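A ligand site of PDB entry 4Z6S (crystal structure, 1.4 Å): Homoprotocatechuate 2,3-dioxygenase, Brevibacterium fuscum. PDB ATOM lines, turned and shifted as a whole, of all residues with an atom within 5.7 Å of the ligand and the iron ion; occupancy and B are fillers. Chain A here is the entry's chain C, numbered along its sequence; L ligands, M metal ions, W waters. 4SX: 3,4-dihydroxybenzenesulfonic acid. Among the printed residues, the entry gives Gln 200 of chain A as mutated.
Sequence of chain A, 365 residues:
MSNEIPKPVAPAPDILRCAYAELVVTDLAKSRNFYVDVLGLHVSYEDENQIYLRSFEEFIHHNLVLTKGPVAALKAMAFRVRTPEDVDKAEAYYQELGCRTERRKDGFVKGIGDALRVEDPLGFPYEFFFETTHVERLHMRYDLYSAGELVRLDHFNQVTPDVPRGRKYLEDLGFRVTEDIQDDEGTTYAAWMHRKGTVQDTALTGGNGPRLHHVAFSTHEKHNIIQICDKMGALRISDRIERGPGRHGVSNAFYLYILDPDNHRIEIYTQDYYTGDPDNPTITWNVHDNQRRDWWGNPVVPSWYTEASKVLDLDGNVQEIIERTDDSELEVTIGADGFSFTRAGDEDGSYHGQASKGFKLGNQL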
ATOM      1  N   HIS A 155     -27.222 -14.783  35.511  1.00  0.00           N
ATOM      2  CA  HIS A 155     -25.856 -14.306  35.262  1.00  0.00           C
ATOM      3  C   HIS A 155     -25.791 -13.164  34.261  1.00  0.00           C
ATOM      4  O   HIS A 155     -26.761 -12.866  33.563  1.00  0.00           O
ATOM      5  CB  HIS A 155     -24.952 -15.466  34.805  1.00  0.00           C
ATOM      6  CG  HIS A 155     -25.294 -16.088  33.486  1.00  0.00           C
ATOM      7  ND1 HIS A 155     -26.075 -17.206  33.410  1.00  0.00           N
ATOM      8  CD2 HIS A 155     -24.884 -15.829  32.227  1.00  0.00           C
ATOM      9  CE1 HIS A 155     -26.167 -17.595  32.141  1.00  0.00           C
ATOM     10  NE2 HIS A 155     -25.474 -16.751  31.398  1.00  0.00           N
ATOM     11  N   ASN A 157     -22.926 -11.874  31.070  1.00  0.00           N
ATOM     12  CA  ASN A 157     -21.813 -12.273  30.229  1.00  0.00           C
ATOM     13  C   ASN A 157     -21.250 -11.031  29.526  1.00  0.00           C
ATOM     14  O   ASN A 157     -21.969 -10.237  28.921  1.00  0.00           O
ATOM     15  CB  ASN A 157     -22.276 -13.299  29.212  1.00  0.00           C
ATOM     16  CG  ASN A 157     -21.135 -13.910  28.427  1.00  0.00           C
ATOM     17  OD1 ASN A 157     -20.409 -13.190  27.741  1.00  0.00           O
ATOM     18  ND2 ASN A 157     -20.971 -15.235  28.525  1.00  0.00           N
ATOM     19  N   ILE A 181     -12.921 -22.288  27.692  1.00  0.00           N
ATOM     20  CA  ILE A 181     -12.680 -22.778  26.341  1.00  0.00           C
ATOM     21  C   ILE A 181     -11.294 -22.291  25.920  1.00  0.00           C
ATOM     22  O   ILE A 181     -11.027 -21.093  25.976  1.00  0.00           O
ATOM     23  CB  ILE A 181     -13.727 -22.253  25.318  1.00  0.00           C
ATOM     24  CG1 ILE A 181     -15.101 -22.832  25.624  1.00  0.00           C
ATOM     25  CG2 ILE A 181     -13.333 -22.614  23.873  1.00  0.00           C
ATOM     26  CD1 ILE A 181     -16.252 -22.208  24.822  1.00  0.00           C
ATOM     27  N   TRP A 192     -16.005 -18.923  32.579  1.00  0.00           N
ATOM     28  CA  TRP A 192     -17.219 -18.802  33.364  1.00  0.00           C
ATOM     29  C   TRP A 192     -16.845 -18.803  34.829  1.00  0.00           C
ATOM     30  O   TRP A 192     -15.997 -19.628  35.239  1.00  0.00           O
ATOM     31  CB  TRP A 192     -18.124 -19.985  33.055  1.00  0.00           C
ATOM     32  CG  TRP A 192     -18.835 -19.897  31.729  1.00  0.00           C
ATOM     33  CD1 TRP A 192     -20.125 -19.593  31.544  1.00  0.00           C
ATOM     34  CD2 TRP A 192     -18.294 -20.192  30.415  1.00  0.00           C
ATOM     35  NE1 TRP A 192     -20.435 -19.618  30.212  1.00  0.00           N
ATOM     36  CE2 TRP A 192     -19.320 -19.974  29.493  1.00  0.00           C
ATOM     37  CE3 TRP A 192     -17.042 -20.598  29.933  1.00  0.00           C
ATOM     38  CZ2 TRP A 192     -19.168 -20.190  28.111  1.00  0.00           C
ATOM     39  CZ3 TRP A 192     -16.863 -20.773  28.562  1.00  0.00           C
ATOM     40  CH2 TRP A 192     -17.932 -20.577  27.662  1.00  0.00           C
ATOM     41  N   GLN A 200     -22.163 -19.921  37.074  1.00  0.00           N
ATOM     42  CA  GLN A 200     -21.727 -18.568  36.825  1.00  0.00           C
ATOM     43  C   GLN A 200     -22.583 -17.496  37.492  1.00  0.00           C
ATOM     44  O   GLN A 200     -23.790 -17.635  37.626  1.00  0.00           O
ATOM     45  CB  GLN A 200     -21.699 -18.312  35.322  1.00  0.00           C
ATOM     46  CG  GLN A 200     -23.014 -18.688  34.664  1.00  0.00           C
ATOM     47  CD  GLN A 200     -22.995 -18.575  33.162  1.00  0.00           C
ATOM     48  OE1 GLN A 200     -22.431 -17.617  32.602  1.00  0.00           O
ATOM     49  NE2 GLN A 200     -23.665 -19.511  32.493  1.00  0.00           N
ATOM     50  N   HIS A 214     -24.738 -10.564  27.234  1.00  0.00           N
ATOM     51  CA  HIS A 214     -26.131 -10.859  27.590  1.00  0.00           C
ATOM     52  C   HIS A 214     -26.378 -10.773  29.057  1.00  0.00           C
ATOM     53  O   HIS A 214     -25.436 -10.805  29.883  1.00  0.00           O
ATOM     54  CB  HIS A 214     -26.601 -12.214  27.026  1.00  0.00           C
ATOM     55  CG  HIS A 214     -25.834 -13.417  27.481  1.00  0.00           C
ATOM     56  ND1 HIS A 214     -24.765 -13.909  26.769  1.00  0.00           N
ATOM     57  CD2 HIS A 214     -26.013 -14.269  28.514  1.00  0.00           C
ATOM     58  CE1 HIS A 214     -24.313 -15.006  27.346  1.00  0.00           C
ATOM     59  NE2 HIS A 214     -25.061 -15.243  28.405  1.00  0.00           N
ATOM     60  N   ALA A 216     -28.864 -13.106  31.635  1.00  0.00           N
ATOM     61  CA  ALA A 216     -29.534 -14.403  31.630  1.00  0.00           C
ATOM     62  C   ALA A 216     -30.493 -14.522  32.784  1.00  0.00           C
ATOM     63  O   ALA A 216     -30.155 -14.231  33.934  1.00  0.00           O
ATOM     64  CB  ALA A 216     -28.534 -15.541  31.674  1.00  0.00           C
ATOM     65  N   ARG A 243     -30.499 -17.370  18.691  1.00  0.00           N
ATOM     66  CA  ARG A 243     -29.723 -18.630  18.765  1.00  0.00           C
ATOM     67  C   ARG A 243     -30.425 -19.578  19.710  1.00  0.00           C
ATOM     68  O   ARG A 243     -30.844 -19.188  20.792  1.00  0.00           O
ATOM     69  CB  ARG A 243     -28.279 -18.368  19.239  1.00  0.00           C
ATOM     70  CG  ARG A 243     -27.449 -19.630  19.458  1.00  0.00           C
ATOM     71  CD  ARG A 243     -26.045 -19.392  20.011  1.00  0.00           C
ATOM     72  NE  ARG A 243     -25.574 -20.691  20.494  1.00  0.00           N
ATOM     73  CZ  ARG A 243     -24.740 -20.917  21.506  1.00  0.00           C
ATOM     74  NH1 ARG A 243     -24.108 -19.934  22.147  1.00  0.00           N
ATOM     75  NH2 ARG A 243     -24.529 -22.164  21.891  1.00  0.00           N
ATOM     76  N   HIS A 248     -26.437 -26.486  26.092  1.00  0.00           N
ATOM     77  CA  HIS A 248     -25.050 -26.038  26.115  1.00  0.00           C
ATOM     78  C   HIS A 248     -24.136 -27.209  26.422  1.00  0.00           C
ATOM     79  O   HIS A 248     -24.503 -28.131  27.119  1.00  0.00           O
ATOM     80  CB  HIS A 248     -24.810 -24.994  27.192  1.00  0.00           C
ATOM     81  CG  HIS A 248     -25.305 -23.619  26.879  1.00  0.00           C
ATOM     82  ND1 HIS A 248     -24.978 -22.956  25.713  1.00  0.00           N
ATOM     83  CD2 HIS A 248     -26.000 -22.730  27.638  1.00  0.00           C
ATOM     84  CE1 HIS A 248     -25.476 -21.725  25.760  1.00  0.00           C
ATOM     85  NE2 HIS A 248     -26.081 -21.560  26.926  1.00  0.00           N
ATOM     86  N   GLY A 249     -22.910 -27.156  25.907  1.00  0.00           N
ATOM     87  CA  GLY A 249     -21.866 -28.053  26.393  1.00  0.00           C
ATOM     88  C   GLY A 249     -21.321 -27.511  27.706  1.00  0.00           C
ATOM     89  O   GLY A 249     -21.617 -28.047  28.785  1.00  0.00           O
ATOM     90  N   VAL A 250     -20.626 -26.387  27.634  1.00  0.00           N
ATOM     91  CA  VAL A 250     -20.290 -25.618  28.823  1.00  0.00           C
ATOM     92  C   VAL A 250     -21.557 -25.335  29.610  1.00  0.00           C
ATOM     93  O   VAL A 250     -22.531 -24.842  29.071  1.00  0.00           O
ATOM     94  CB  VAL A 250     -19.623 -24.288  28.462  1.00  0.00           C
ATOM     95  CG1 VAL A 250     -19.426 -23.403  29.697  1.00  0.00           C
ATOM     96  CG2 VAL A 250     -18.305 -24.500  27.755  1.00  0.00           C
ATOM     97  N   SER A 251     -21.542 -25.696  30.880  1.00  0.00           N
ATOM     98  CA  SER A 251     -22.656 -25.450  31.840  1.00  0.00           C
ATOM     99  C   SER A 251     -23.725 -26.560  31.867  1.00  0.00           C
ATOM    100  O   SER A 251     -24.442 -26.669  32.872  1.00  0.00           O
ATOM    101  CB  SER A 251     -23.342 -24.081  31.685  1.00  0.00           C
ATOM    102  OG  SER A 251     -24.398 -24.125  30.710  1.00  0.00           O
ATOM    103  N   TYR A 255     -30.982 -23.739  26.888  1.00  0.00           N
ATOM    104  CA  TYR A 255     -30.806 -22.298  26.642  1.00  0.00           C
ATOM    105  C   TYR A 255     -31.547 -21.796  25.406  1.00  0.00           C
ATOM    106  O   TYR A 255     -31.923 -22.567  24.512  1.00  0.00           O
ATOM    107  CB  TYR A 255     -29.322 -21.970  26.482  1.00  0.00           C
ATOM    108  CG  TYR A 255     -28.755 -22.396  25.147  1.00  0.00           C
ATOM    109  CD1 TYR A 255     -28.847 -21.575  24.034  1.00  0.00           C
ATOM    110  CD2 TYR A 255     -28.158 -23.622  24.994  1.00  0.00           C
ATOM    111  CE1 TYR A 255     -28.317 -21.961  22.807  1.00  0.00           C
ATOM    112  CE2 TYR A 255     -27.638 -24.018  23.776  1.00  0.00           C
ATOM    113  CZ  TYR A 255     -27.745 -23.204  22.681  1.00  0.00           C
ATOM    114  OH  TYR A 255     -27.211 -23.592  21.445  1.00  0.00           O
ATOM    115  N   TYR A 257     -31.313 -17.699  23.185  1.00  0.00           N
ATOM    116  CA  TYR A 257     -30.972 -16.284  23.136  1.00  0.00           C
ATOM    117  C   TYR A 257     -31.953 -15.500  22.260  1.00  0.00           C
ATOM    118  O   TYR A 257     -32.204 -15.884  21.103  1.00  0.00           O
ATOM    119  CB  TYR A 257     -29.542 -16.048  22.622  1.00  0.00           C
ATOM    120  CG  TYR A 257     -28.477 -16.745  23.420  1.00  0.00           C
ATOM    121  CD1 TYR A 257     -28.102 -18.057  23.122  1.00  0.00           C
ATOM    122  CD2 TYR A 257     -27.849 -16.110  24.486  1.00  0.00           C
ATOM    123  CE1 TYR A 257     -27.115 -18.701  23.840  1.00  0.00           C
ATOM    124  CE2 TYR A 257     -26.866 -16.752  25.213  1.00  0.00           C
ATOM    125  CZ  TYR A 257     -26.509 -18.037  24.878  1.00  0.00           C
ATOM    126  OH  TYR A 257     -25.527 -18.696  25.588  1.00  0.00           O
ATOM    127  N   GLU A 267     -30.563 -14.095  27.525  1.00  0.00           N
ATOM    128  CA  GLU A 267     -30.525 -15.578  27.524  1.00  0.00           C
ATOM    129  C   GLU A 267     -31.559 -16.092  28.518  1.00  0.00           C
ATOM    130  O   GLU A 267     -31.761 -15.485  29.598  1.00  0.00           O
ATOM    131  CB  GLU A 267     -29.151 -16.122  27.929  1.00  0.00           C
ATOM    132  CG  GLU A 267     -29.050 -17.637  27.829  1.00  0.00           C
ATOM    133  CD  GLU A 267     -27.723 -18.186  28.249  1.00  0.00           C
ATOM    134  OE1 GLU A 267     -26.945 -17.429  28.865  1.00  0.00           O
ATOM    135  OE2 GLU A 267     -27.445 -19.360  27.908  1.00  0.00           O
ATOM    136  N   TYR A 269     -32.332 -19.755  30.448  1.00  0.00           N
ATOM    137  CA  TYR A 269     -31.347 -20.735  30.888  1.00  0.00           C
ATOM    138  C   TYR A 269     -31.944 -21.610  31.979  1.00  0.00           C
ATOM    139  O   TYR A 269     -32.655 -21.127  32.851  1.00  0.00           O
ATOM    140  CB  TYR A 269     -30.172 -19.902  31.424  1.00  0.00           C
ATOM    141  CG  TYR A 269     -28.924 -20.532  31.966  1.00  0.00           C
ATOM    142  CD1 TYR A 269     -27.810 -20.700  31.164  1.00  0.00           C
ATOM    143  CD2 TYR A 269     -28.816 -20.832  33.292  1.00  0.00           C
ATOM    144  CE1 TYR A 269     -26.614 -21.178  31.679  1.00  0.00           C
ATOM    145  CE2 TYR A 269     -27.630 -21.336  33.799  1.00  0.00           C
ATOM    146  CZ  TYR A 269     -26.534 -21.510  32.991  1.00  0.00           C
ATOM    147  OH  TYR A 269     -25.312 -21.953  33.529  1.00  0.00           O
ATOM    148  N   ARG A 292     -19.186 -28.092  22.235  1.00  0.00           N
ATOM    149  CA  ARG A 292     -18.842 -27.311  23.424  1.00  0.00           C
ATOM    150  C   ARG A 292     -19.873 -26.227  23.738  1.00  0.00           C
ATOM    151  O   ARG A 292     -20.107 -25.919  24.907  1.00  0.00           O
ATOM    152  CB  ARG A 292     -17.437 -26.656  23.288  1.00  0.00           C
ATOM    153  CG  ARG A 292     -17.426 -25.406  22.381  1.00  0.00           C
ATOM    154  CD  ARG A 292     -16.073 -25.003  21.836  1.00  0.00           C
ATOM    155  NE  ARG A 292     -16.263 -23.805  20.994  1.00  0.00           N
ATOM    156  CZ  ARG A 292     -16.761 -23.823  19.761  1.00  0.00           C
ATOM    157  NH1 ARG A 292     -17.046 -24.985  19.176  1.00  0.00           N
ATOM    158  NH2 ARG A 292     -16.960 -22.706  19.093  1.00  0.00           N
ATOM    159  N   ARG A 293     -20.458 -25.615  22.691  1.00  0.00           N
ATOM    160  CA  ARG A 293     -21.413 -24.531  22.869  1.00  0.00           C
ATOM    161  C   ARG A 293     -22.839 -24.970  22.650  1.00  0.00           C
ATOM    162  O   ARG A 293     -23.727 -24.614  23.450  1.00  0.00           O
ATOM    163  CB  ARG A 293     -21.077 -23.324  21.984  1.00  0.00           C
ATOM    164  CG  ARG A 293     -19.769 -22.591  22.344  1.00  0.00           C
ATOM    165  CD  ARG A 293     -19.836 -21.116  22.001  1.00  0.00           C
ATOM    166  NE  ARG A 293     -18.670 -20.339  22.414  1.00  0.00           N
ATOM    167  CZ  ARG A 293     -18.595 -19.575  23.498  1.00  0.00           C
ATOM    168  NH1 ARG A 293     -19.597 -19.495  24.381  1.00  0.00           N
ATOM    169  NH2 ARG A 293     -17.510 -18.862  23.717  1.00  0.00           N
ATOM    170  N   ASP A 294     -23.064 -25.743  21.596  1.00  0.00           N
ATOM    171  CA  ASP A 294     -24.301 -26.479  21.466  1.00  0.00           C
ATOM    172  C   ASP A 294     -23.941 -27.964  21.453  1.00  0.00           C
ATOM    173  O   ASP A 294     -23.272 -28.448  20.542  1.00  0.00           O
ATOM    174  CB  ASP A 294     -25.083 -26.076  20.217  1.00  0.00           C
ATOM    175  CG  ASP A 294     -26.457 -26.713  20.171  1.00  0.00           C
ATOM    176  OD1 ASP A 294     -27.384 -26.142  20.809  1.00  0.00           O
ATOM    177  OD2 ASP A 294     -26.587 -27.810  19.554  1.00  0.00           O
ATOM    178  N   TRP A 304     -23.872 -13.992  17.122  1.00  0.00           N
ATOM    179  CA  TRP A 304     -23.615 -14.320  18.526  1.00  0.00           C
ATOM    180  C   TRP A 304     -22.181 -14.013  18.918  1.00  0.00           C
ATOM    181  O   TRP A 304     -21.893 -13.619  20.054  1.00  0.00           O
ATOM    182  CB  TRP A 304     -23.972 -15.793  18.818  1.00  0.00           C
ATOM    183  CG  TRP A 304     -24.208 -16.075  20.277  1.00  0.00           C
ATOM    184  CD1 TRP A 304     -25.388 -15.987  20.951  1.00  0.00           C
ATOM    185  CD2 TRP A 304     -23.227 -16.496  21.234  1.00  0.00           C
ATOM    186  NE1 TRP A 304     -25.209 -16.328  22.272  1.00  0.00           N
ATOM    187  CE2 TRP A 304     -23.901 -16.666  22.472  1.00  0.00           C
ATOM    188  CE3 TRP A 304     -21.863 -16.743  21.166  1.00  0.00           C
ATOM    189  CZ2 TRP A 304     -23.231 -17.046  23.637  1.00  0.00           C
ATOM    190  CZ3 TRP A 304     -21.224 -17.131  22.298  1.00  0.00           C
ATOM    191  CH2 TRP A 304     -21.894 -17.270  23.529  1.00  0.00           C
HETATM  192  O11 4SX L   1     -22.673 -21.429  24.265  1.00  0.00           O
HETATM  193  S9  4SX L   1     -21.920 -22.002  25.570  1.00  0.00           S
HETATM  194  O12 4SX L   1     -22.164 -23.443  25.855  1.00  0.00           O
HETATM  195  O10 4SX L   1     -20.498 -21.704  25.392  1.00  0.00           O
HETATM  196  C4  4SX L   1     -22.507 -21.104  26.905  1.00  0.00           C
HETATM  197  C3  4SX L   1     -22.950 -19.791  26.663  1.00  0.00           C
HETATM  198  C5  4SX L   1     -22.692 -21.734  28.143  1.00  0.00           C
HETATM  199  C6  4SX L   1     -23.301 -21.053  29.181  1.00  0.00           C
HETATM  200  C1  4SX L   1     -23.786 -19.755  28.949  1.00  0.00           C
HETATM  201  O7  4SX L   1     -24.457 -19.039  29.909  1.00  0.00           O
HETATM  202  C2  4SX L   1     -23.599 -19.119  27.699  1.00  0.00           C
HETATM  203  O8  4SX L   1     -24.100 -17.867  27.562  1.00  0.00           O
HETATM  204 FE    FE M   1     -24.993 -17.220  29.316  1.00  0.00          FE
HETATM  205  O   HOH W   1     -22.696 -16.848  29.998  1.00  0.00           O
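Water W1 lies within hydrogen-bond range of OE1 of Gln 200 (2.7 Å) and ND2 of Asn 157 (2.8 Å).
O of Arg 292 lies close to O12 of the ligand.
NE1 of Trp 192 touches C6 of the ligand, 3.4 Å away.
Gly 249 touches the ligand.
O of Val 250 touches C5 of the ligand, 3.2 Å away.
OG of Ser 251 touches C6 of the ligand, 3.6 Å away.
Tyr 269 touches the ligand (CE1 to O7, 3.5 Å).
Hydrophobic or aromatic side chains that line the ligand: His 155, Trp 192, His 214, His 248, Val 250, Tyr 257 and Tyr 269.
14 residues have an atom within 4 Å of the ligand: His 155, Trp 192, Gln 200, His 214, Arg 243, His 248, Gly 249, Val 250, Ser 251, Tyr 257, Glu 267, Tyr 269, Arg 292 and Arg 293.
The nearest printed residue that does not touch the ligand is Trp 304 (4.1 Å).
Within 4 Å of the iron ion: His 155, His 214 and Glu 267.
The side-chain carboxylate of Glu 267 is in hydrogen-bond range of the side-chain hydroxyl of Tyr 257 (3.1 Å).
The backbone carbonyl oxygen (O) of His 214 lies within hydrogen-bond range of the backbone NH (N) of Asn 157.
A ring nitrogen (ND1) of His 155 sits close to the side-chain amide nitrogen (NE2) of Gln 200 (3.5 Å).
The backbone NH (N) of Ala 216 sits at hydrogen-bond distance from the backbone carbonyl oxygen (O) of His 155 (2.9 Å).
A ring nitrogen (NE2) of His 248 sits close to the side-chain hydroxyl (OH) of Tyr 257 (3.2 Å).
NH2 of Arg 243 sits at hydrogen-bond distance from O of Arg 293.
The side-chain hydroxyl of Tyr 269 lies within hydrogen-bond range of the side-chain amide nitrogen of Gln 200 (3.1 Å).
The backbone carbonyl oxygen of Arg 292 is in hydrogen-bond range of the backbone NH of Val 250 (2.8 Å).
The iron ion is bound by an oxygen (O7) of the ligand (2.0 Å), the side-chain carboxylate of Glu 267 (2.0 Å), an oxygen (O8) of the ligand (2.1 Å), a ring nitrogen (NE2) of His 214 (2.2 Å), a ring nitrogen (NE2) of His 155 (2.2 Å) and water W1 (2.4 Å).
The iron ion has six donor atoms within binding distance.
O8 of the ligand sits close to OH of Tyr 257 (2.6 Å).
O of Arg 293 sits close to O12 of the ligand, at 3.1 Å.
NH1 of Arg 293 lies within salt-bridge range of O10 of the ligand (2.6 Å).
The side-chain amide nitrogen (NE2) of Gln 200 lies close to an oxygen (O7) of the ligand, 2.7 Å away.
O12 of the ligand lies within hydrogen-bond range of ND1 of His 248, 2.9 Å away.
The guanidinium group (NH1) of Arg 243 is in salt-bridge range of an oxygen (O11) of the ligand.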
